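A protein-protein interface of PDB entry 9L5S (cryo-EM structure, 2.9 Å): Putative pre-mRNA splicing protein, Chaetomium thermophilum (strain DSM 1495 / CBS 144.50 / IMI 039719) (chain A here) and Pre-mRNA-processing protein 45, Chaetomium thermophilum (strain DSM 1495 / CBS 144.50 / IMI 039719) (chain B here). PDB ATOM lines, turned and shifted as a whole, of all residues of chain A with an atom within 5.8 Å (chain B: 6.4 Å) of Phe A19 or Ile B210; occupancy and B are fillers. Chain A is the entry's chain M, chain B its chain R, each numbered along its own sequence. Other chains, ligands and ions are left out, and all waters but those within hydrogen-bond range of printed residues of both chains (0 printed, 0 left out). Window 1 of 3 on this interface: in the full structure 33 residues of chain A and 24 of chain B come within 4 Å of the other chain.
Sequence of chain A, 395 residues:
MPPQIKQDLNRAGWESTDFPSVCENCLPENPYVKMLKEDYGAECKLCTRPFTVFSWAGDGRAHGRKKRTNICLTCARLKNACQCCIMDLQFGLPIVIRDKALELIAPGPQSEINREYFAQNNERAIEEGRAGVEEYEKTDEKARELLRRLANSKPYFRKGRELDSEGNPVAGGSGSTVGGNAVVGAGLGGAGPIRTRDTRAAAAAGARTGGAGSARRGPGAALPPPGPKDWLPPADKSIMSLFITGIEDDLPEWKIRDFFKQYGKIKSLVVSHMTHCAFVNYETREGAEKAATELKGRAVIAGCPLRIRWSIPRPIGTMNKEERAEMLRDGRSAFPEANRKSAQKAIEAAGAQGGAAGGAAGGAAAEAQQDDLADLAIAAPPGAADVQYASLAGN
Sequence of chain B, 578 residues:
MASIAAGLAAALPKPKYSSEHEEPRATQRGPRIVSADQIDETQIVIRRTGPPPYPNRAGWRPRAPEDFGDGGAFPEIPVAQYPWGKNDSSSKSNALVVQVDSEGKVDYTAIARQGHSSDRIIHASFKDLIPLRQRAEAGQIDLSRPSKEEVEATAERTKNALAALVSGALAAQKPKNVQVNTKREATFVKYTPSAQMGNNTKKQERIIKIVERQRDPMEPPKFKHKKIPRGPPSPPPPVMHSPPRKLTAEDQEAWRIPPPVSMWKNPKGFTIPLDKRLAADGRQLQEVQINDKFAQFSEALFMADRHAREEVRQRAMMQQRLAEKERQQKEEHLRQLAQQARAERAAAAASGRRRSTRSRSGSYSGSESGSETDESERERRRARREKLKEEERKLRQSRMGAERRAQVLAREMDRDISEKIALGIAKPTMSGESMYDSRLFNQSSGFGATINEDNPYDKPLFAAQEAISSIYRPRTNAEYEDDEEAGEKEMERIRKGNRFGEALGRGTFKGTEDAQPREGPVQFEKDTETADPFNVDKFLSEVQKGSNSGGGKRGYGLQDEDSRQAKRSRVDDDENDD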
ATOM      1  N   ASP A  18     -13.982  11.468  30.280  1.00  0.00           N
ATOM      2  CA  ASP A  18     -14.721  10.377  29.656  1.00  0.00           C
ATOM      3  C   ASP A  18     -16.159  10.792  29.366  1.00  0.00           C
ATOM      4  O   ASP A  18     -16.982   9.973  28.962  1.00  0.00           O
ATOM      5  CB  ASP A  18     -14.700   9.134  30.548  1.00  0.00           C
ATOM      6  CG  ASP A  18     -13.369   8.412  30.508  1.00  0.00           C
ATOM      7  OD1 ASP A  18     -12.702   8.452  29.453  1.00  0.00           O
ATOM      8  OD2 ASP A  18     -12.985   7.808  31.532  1.00  0.00           O
ATOM      9  N   PHE A  19     -16.453  12.076  29.575  1.00  0.00           N
ATOM     10  CA  PHE A  19     -17.777  12.618  29.337  1.00  0.00           C
ATOM     11  C   PHE A  19     -17.626  14.044  28.833  1.00  0.00           C
ATOM     12  O   PHE A  19     -16.829  14.809  29.396  1.00  0.00           O
ATOM     13  CB  PHE A  19     -18.634  12.593  30.607  1.00  0.00           C
ATOM     14  CG  PHE A  19     -20.079  12.905  30.366  1.00  0.00           C
ATOM     15  CD1 PHE A  19     -20.909  11.985  29.747  1.00  0.00           C
ATOM     16  CD2 PHE A  19     -20.607  14.124  30.750  1.00  0.00           C
ATOM     17  CE1 PHE A  19     -22.237  12.278  29.519  1.00  0.00           C
ATOM     18  CE2 PHE A  19     -21.930  14.421  30.523  1.00  0.00           C
ATOM     19  CZ  PHE A  19     -22.748  13.498  29.910  1.00  0.00           C
ATOM     20  N   PRO A  20     -18.358  14.430  27.794  1.00  0.00           N
ATOM     21  CA  PRO A  20     -18.208  15.776  27.238  1.00  0.00           C
ATOM     22  C   PRO A  20     -18.890  16.832  28.096  1.00  0.00           C
ATOM     23  O   PRO A  20     -19.721  16.540  28.957  1.00  0.00           O
ATOM     24  CB  PRO A  20     -18.893  15.656  25.873  1.00  0.00           C
ATOM     25  CG  PRO A  20     -19.974  14.664  26.131  1.00  0.00           C
ATOM     26  CD  PRO A  20     -19.316  13.632  27.011  1.00  0.00           C
ATOM     27  N   SER A  21     -18.526  18.082  27.834  1.00  0.00           N
ATOM     28  CA  SER A  21     -19.119  19.236  28.502  1.00  0.00           C
ATOM     29  C   SER A  21     -19.917  19.985  27.441  1.00  0.00           C
ATOM     30  O   SER A  21     -19.407  20.886  26.775  1.00  0.00           O
ATOM     31  CB  SER A  21     -18.058  20.120  29.138  1.00  0.00           C
ATOM     32  OG  SER A  21     -17.207  20.676  28.157  1.00  0.00           O
ATOM     33  N   VAL A  33     -30.201  10.262  25.443  1.00  0.00           N
ATOM     34  CA  VAL A  33     -29.260  10.627  24.392  1.00  0.00           C
ATOM     35  C   VAL A  33     -28.470   9.388  23.997  1.00  0.00           C
ATOM     36  O   VAL A  33     -27.830   8.754  24.843  1.00  0.00           O
ATOM     37  CB  VAL A  33     -28.318  11.753  24.843  1.00  0.00           C
ATOM     38  CG1 VAL A  33     -27.584  12.345  23.650  1.00  0.00           C
ATOM     39  CG2 VAL A  33     -29.093  12.828  25.587  1.00  0.00           C
ATOM     40  N   MET A  35     -25.257   8.360  22.146  1.00  0.00           N
ATOM     41  CA  MET A  35     -24.034   9.105  21.889  1.00  0.00           C
ATOM     42  C   MET A  35     -22.924   8.163  21.443  1.00  0.00           C
ATOM     43  O   MET A  35     -22.723   7.099  22.034  1.00  0.00           O
ATOM     44  CB  MET A  35     -23.609   9.875  23.146  1.00  0.00           C
ATOM     45  CG  MET A  35     -22.417  10.793  22.968  1.00  0.00           C
ATOM     46  SD  MET A  35     -22.163  11.816  24.431  1.00  0.00           S
ATOM     47  CE  MET A  35     -23.381  13.099  24.168  1.00  0.00           C
ATOM     48  N   LEU A  36     -22.216   8.559  20.389  1.00  0.00           N
ATOM     49  CA  LEU A  36     -21.038   7.856  19.907  1.00  0.00           C
ATOM     50  C   LEU A  36     -19.786   8.510  20.475  1.00  0.00           C
ATOM     51  O   LEU A  36     -19.744   9.727  20.663  1.00  0.00           O
ATOM     52  CB  LEU A  36     -20.984   7.869  18.378  1.00  0.00           C
ATOM     53  CG  LEU A  36     -21.932   6.922  17.642  1.00  0.00           C
ATOM     54  CD1 LEU A  36     -22.007   7.288  16.172  1.00  0.00           C
ATOM     55  CD2 LEU A  36     -21.488   5.482  17.813  1.00  0.00           C
ATOM     56  N   LYS A  37     -18.767   7.698  20.744  1.00  0.00           N
ATOM     57  CA  LYS A  37     -17.519   8.170  21.328  1.00  0.00           C
ATOM     58  C   LYS A  37     -16.349   7.596  20.545  1.00  0.00           C
ATOM     59  O   LYS A  37     -16.264   6.379  20.356  1.00  0.00           O
ATOM     60  CB  LYS A  37     -17.421   7.771  22.804  1.00  0.00           C
ATOM     61  CG  LYS A  37     -16.013   7.773  23.365  1.00  0.00           C
ATOM     62  CD  LYS A  37     -15.964   7.113  24.729  1.00  0.00           C
ATOM     63  CE  LYS A  37     -14.538   7.018  25.243  1.00  0.00           C
ATOM     64  NZ  LYS A  37     -14.482   6.506  26.638  1.00  0.00           N
ATOM     65  N   PHE A  54     -17.099  13.191  21.056  1.00  0.00           N
ATOM     66  CA  PHE A  54     -18.428  12.671  21.331  1.00  0.00           C
ATOM     67  C   PHE A  54     -19.397  13.267  20.323  1.00  0.00           C
ATOM     68  O   PHE A  54     -19.348  14.467  20.042  1.00  0.00           O
ATOM     69  CB  PHE A  54     -18.871  13.010  22.757  1.00  0.00           C
ATOM     70  CG  PHE A  54     -18.147  12.234  23.816  1.00  0.00           C
ATOM     71  CD1 PHE A  54     -16.915  12.661  24.283  1.00  0.00           C
ATOM     72  CD2 PHE A  54     -18.686  11.071  24.335  1.00  0.00           C
ATOM     73  CE1 PHE A  54     -16.243  11.952  25.255  1.00  0.00           C
ATOM     74  CE2 PHE A  54     -18.015  10.354  25.307  1.00  0.00           C
ATOM     75  CZ  PHE A  54     -16.792  10.796  25.766  1.00  0.00           C
ATOM     76  N   LEU A  73     -11.532  19.205  25.873  1.00  0.00           N
ATOM     77  CA  LEU A  73     -12.049  19.586  27.182  1.00  0.00           C
ATOM     78  C   LEU A  73     -11.156  20.617  27.864  1.00  0.00           C
ATOM     79  O   LEU A  73     -11.652  21.476  28.601  1.00  0.00           O
ATOM     80  CB  LEU A  73     -12.211  18.344  28.057  1.00  0.00           C
ATOM     81  CG  LEU A  73     -13.012  18.503  29.349  1.00  0.00           C
ATOM     82  CD1 LEU A  73     -14.394  19.056  29.061  1.00  0.00           C
ATOM     83  CD2 LEU A  73     -13.108  17.177  30.077  1.00  0.00           C
ATOM     84  N   GLN A  83     -18.441  22.452  24.166  1.00  0.00           N
ATOM     85  CA  GLN A  83     -17.548  21.803  23.217  1.00  0.00           C
ATOM     86  C   GLN A  83     -18.128  21.759  21.809  1.00  0.00           C
ATOM     87  O   GLN A  83     -17.372  21.586  20.848  1.00  0.00           O
ATOM     88  CB  GLN A  83     -17.227  20.393  23.704  1.00  0.00           C
ATOM     89  CG  GLN A  83     -16.022  20.317  24.620  1.00  0.00           C
ATOM     90  CD  GLN A  83     -15.655  18.894  24.972  1.00  0.00           C
ATOM     91  OE1 GLN A  83     -16.241  18.297  25.874  1.00  0.00           O
ATOM     92  NE2 GLN A  83     -14.685  18.339  24.259  1.00  0.00           N
ATOM     93  N   GLU B 185     -19.844  -2.728  24.115  1.00  0.00           N
ATOM     94  CA  GLU B 185     -20.838  -2.637  25.174  1.00  0.00           C
ATOM     95  C   GLU B 185     -21.046  -1.181  25.572  1.00  0.00           C
ATOM     96  O   GLU B 185     -20.080  -0.442  25.786  1.00  0.00           O
ATOM     97  CB  GLU B 185     -20.414  -3.467  26.384  1.00  0.00           C
ATOM     98  CG  GLU B 185     -21.536  -3.720  27.376  1.00  0.00           C
ATOM     99  CD  GLU B 185     -21.202  -4.817  28.366  1.00  0.00           C
ATOM    100  OE1 GLU B 185     -20.112  -5.415  28.248  1.00  0.00           O
ATOM    101  OE2 GLU B 185     -22.034  -5.085  29.258  1.00  0.00           O
ATOM    102  N   ALA B 186     -22.307  -0.774  25.669  1.00  0.00           N
ATOM    103  CA  ALA B 186     -22.650   0.608  25.952  1.00  0.00           C
ATOM    104  C   ALA B 186     -22.397   0.951  27.417  1.00  0.00           C
ATOM    105  O   ALA B 186     -22.394   0.088  28.298  1.00  0.00           O
ATOM    106  CB  ALA B 186     -24.112   0.878  25.602  1.00  0.00           C
ATOM    107  N   THR B 187     -22.182   2.240  27.665  1.00  0.00           N
ATOM    108  CA  THR B 187     -22.015   2.778  29.008  1.00  0.00           C
ATOM    109  C   THR B 187     -23.116   3.798  29.258  1.00  0.00           C
ATOM    110  O   THR B 187     -23.323   4.701  28.444  1.00  0.00           O
ATOM    111  CB  THR B 187     -20.634   3.422  29.176  1.00  0.00           C
ATOM    112  OG1 THR B 187     -19.617   2.429  28.998  1.00  0.00           O
ATOM    113  CG2 THR B 187     -20.485   4.036  30.558  1.00  0.00           C
ATOM    114  N   PHE B 188     -23.822   3.660  30.373  1.00  0.00           N
ATOM    115  CA  PHE B 188     -24.941   4.538  30.679  1.00  0.00           C
ATOM    116  C   PHE B 188     -24.522   5.554  31.731  1.00  0.00           C
ATOM    117  O   PHE B 188     -23.870   5.207  32.720  1.00  0.00           O
ATOM    118  CB  PHE B 188     -26.151   3.738  31.158  1.00  0.00           C
ATOM    119  CG  PHE B 188     -26.717   2.822  30.111  1.00  0.00           C
ATOM    120  CD1 PHE B 188     -27.614   3.294  29.168  1.00  0.00           C
ATOM    121  CD2 PHE B 188     -26.351   1.486  30.073  1.00  0.00           C
ATOM    122  CE1 PHE B 188     -28.135   2.451  28.206  1.00  0.00           C
ATOM    123  CE2 PHE B 188     -26.870   0.639  29.114  1.00  0.00           C
ATOM    124  CZ  PHE B 188     -27.762   1.122  28.180  1.00  0.00           C
ATOM    125  N   VAL B 189     -24.888   6.812  31.502  1.00  0.00           N
ATOM    126  CA  VAL B 189     -24.474   7.927  32.345  1.00  0.00           C
ATOM    127  C   VAL B 189     -25.718   8.682  32.791  1.00  0.00           C
ATOM    128  O   VAL B 189     -26.568   9.028  31.964  1.00  0.00           O
ATOM    129  CB  VAL B 189     -23.503   8.868  31.602  1.00  0.00           C
ATOM    130  CG1 VAL B 189     -23.219  10.116  32.419  1.00  0.00           C
ATOM    131  CG2 VAL B 189     -22.204   8.151  31.279  1.00  0.00           C
ATOM    132  N   TYR B 191     -26.774  12.084  33.860  1.00  0.00           N
ATOM    133  CA  TYR B 191     -26.236  13.430  33.727  1.00  0.00           C
ATOM    134  C   TYR B 191     -27.278  14.435  34.196  1.00  0.00           C
ATOM    135  O   TYR B 191     -28.343  14.558  33.583  1.00  0.00           O
ATOM    136  CB  TYR B 191     -25.837  13.704  32.278  1.00  0.00           C
ATOM    137  CG  TYR B 191     -25.472  15.138  31.998  1.00  0.00           C
ATOM    138  CD1 TYR B 191     -24.370  15.725  32.603  1.00  0.00           C
ATOM    139  CD2 TYR B 191     -26.232  15.909  31.130  1.00  0.00           C
ATOM    140  CE1 TYR B 191     -24.033  17.035  32.347  1.00  0.00           C
ATOM    141  CE2 TYR B 191     -25.905  17.219  30.870  1.00  0.00           C
ATOM    142  CZ  TYR B 191     -24.805  17.777  31.482  1.00  0.00           C
ATOM    143  OH  TYR B 191     -24.476  19.082  31.223  1.00  0.00           O
ATOM    144  N   ILE B 208     -27.858   8.949  29.374  1.00  0.00           N
ATOM    145  CA  ILE B 208     -27.093   9.048  28.139  1.00  0.00           C
ATOM    146  C   ILE B 208     -26.407   7.717  27.877  1.00  0.00           C
ATOM    147  O   ILE B 208     -25.679   7.203  28.735  1.00  0.00           O
ATOM    148  CB  ILE B 208     -26.076  10.200  28.193  1.00  0.00           C
ATOM    149  CG1 ILE B 208     -26.811  11.531  28.369  1.00  0.00           C
ATOM    150  CG2 ILE B 208     -25.223  10.225  26.936  1.00  0.00           C
ATOM    151  CD1 ILE B 208     -25.913  12.736  28.418  1.00  0.00           C
ATOM    152  N   LYS B 209     -26.654   7.158  26.695  1.00  0.00           N
ATOM    153  CA  LYS B 209     -26.000   5.942  26.232  1.00  0.00           C
ATOM    154  C   LYS B 209     -24.772   6.327  25.415  1.00  0.00           C
ATOM    155  O   LYS B 209     -24.893   7.013  24.396  1.00  0.00           O
ATOM    156  CB  LYS B 209     -26.970   5.112  25.393  1.00  0.00           C
ATOM    157  CG  LYS B 209     -26.494   3.718  25.034  1.00  0.00           C
ATOM    158  CD  LYS B 209     -27.575   2.973  24.267  1.00  0.00           C
ATOM    159  CE  LYS B 209     -27.010   1.788  23.505  1.00  0.00           C
ATOM    160  NZ  LYS B 209     -28.083   0.938  22.921  1.00  0.00           N
ATOM    161  N   ILE B 210     -23.598   5.890  25.858  1.00  0.00           N
ATOM    162  CA  ILE B 210     -22.336   6.200  25.202  1.00  0.00           C
ATOM    163  C   ILE B 210     -21.770   4.901  24.652  1.00  0.00           C
ATOM    164  O   ILE B 210     -21.492   3.964  25.414  1.00  0.00           O
ATOM    165  CB  ILE B 210     -21.344   6.876  26.160  1.00  0.00           C
ATOM    166  CG1 ILE B 210     -21.945   8.169  26.717  1.00  0.00           C
ATOM    167  CG2 ILE B 210     -20.028   7.150  25.453  1.00  0.00           C
ATOM    168  CD1 ILE B 210     -21.003   8.957  27.598  1.00  0.00           C
ATOM    169  N   VAL B 211     -21.607   4.844  23.333  1.00  0.00           N
ATOM    170  CA  VAL B 211     -21.116   3.668  22.631  1.00  0.00           C
ATOM    171  C   VAL B 211     -19.877   4.079  21.848  1.00  0.00           C
ATOM    172  O   VAL B 211     -19.819   5.177  21.288  1.00  0.00           O
ATOM    173  CB  VAL B 211     -22.200   3.079  21.693  1.00  0.00           C
ATOM    174  CG1 VAL B 211     -21.713   1.815  21.002  1.00  0.00           C
ATOM    175  CG2 VAL B 211     -23.486   2.808  22.452  1.00  0.00           C
ATOM    176  N   GLU B 212     -18.869   3.210  21.841  1.00  0.00           N
ATOM    177  CA  GLU B 212     -17.714   3.424  20.982  1.00  0.00           C
ATOM    178  C   GLU B 212     -18.139   3.367  19.517  1.00  0.00           C
ATOM    179  O   GLU B 212     -18.994   2.569  19.127  1.00  0.00           O
ATOM    180  CB  GLU B 212     -16.637   2.376  21.270  1.00  0.00           C
ATOM    181  CG  GLU B 212     -15.349   2.554  20.483  1.00  0.00           C
ATOM    182  CD  GLU B 212     -14.297   1.522  20.841  1.00  0.00           C
ATOM    183  OE1 GLU B 212     -14.581   0.651  21.689  1.00  0.00           O
ATOM    184  OE2 GLU B 212     -13.186   1.584  20.275  1.00  0.00           O
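Of the 11 printed residues of chain B, 7 touch a printed residue of chain A. Hydrophobic or aromatic side chains of chain B within 4 Å of the printed part of chain A: Val B189, Tyr B191, Ile B208 and Ile B210. Printed residues of chain A that touch a printed residue of chain B: Phe A19, Val A33, Met A35, Leu A36, Lys A37 and Phe A54. Hydrophobic or aromatic side chains of chain A within 4 Å of the printed part of chain B: Phe A19, Val A33, Met A35, Leu A36 and Phe A54. Among the printed residues, 14 pairs touch across the chains. Among the printed residues, no Asp or Glu carboxylate lies within 4 Å of a Lys or Arg side-chain nitrogen of the other chain.
Printed residues of chain B within 4 Å of Phe A54: Ile B210. Of the printed residues of chain A, Lys B209 touches Val A33 (2.7 Å) and Met A35 (2.6 Å). Phe B188 touches none of the printed residues of chain A. Ser A21 touches none of the printed residues of chain B. The nearest residue of chain A that does not touch Ile B210 is Asp A18 (4.4 Å).
Among the printed residues, merely in contact across the chains: Leu A36 with Val B211 (3.3 Å), Met A35 with Ile B210 (3.3 Å), Lys A37 with Glu B212 (3.4 Å), Val A33 with Ile B208 (3.4 Å), Phe A19 with Tyr B191 (3.5 Å), Phe A19 with Ile B208 (3.6 Å), Phe A19 with Ile B210 (3.7 Å), Phe A19 with Val B189 (3.7 Å), Lys A37 with Ile B210 (3.8 Å) and Phe A54 with Ile B210 (3.8 Å).
The backbone carbonyl oxygen (O) of Lys B209 lies within hydrogen-bond range of the backbone NH (N) of Met A35, at 2.6 Å. The backbone NH (N) of Lys A37 is in hydrogen-bond range of the backbone carbonyl oxygen (O) of Val B211. The backbone carbonyl oxygen (O) of Met A35 lies within hydrogen-bond range of the backbone NH (N) of Val B211. The backbone carbonyl oxygen (O) of Val A33 lies within hydrogen-bond range of the backbone NH (N) of Lys B209 (2.7 Å).
The backbone NH (N) of Ile B210 lies within hydrogen-bond range of the backbone carbonyl oxygen (O) of Thr B187, at 2.9 Å. The side-chain carboxylate (OD1) of Asp A18 lies within salt-bridge range of the side-chain amino group (NZ) of Lys A37 (3.9 Å). N of Ile B208 lies within hydrogen-bond range of O of Val B189 (2.9 Å).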
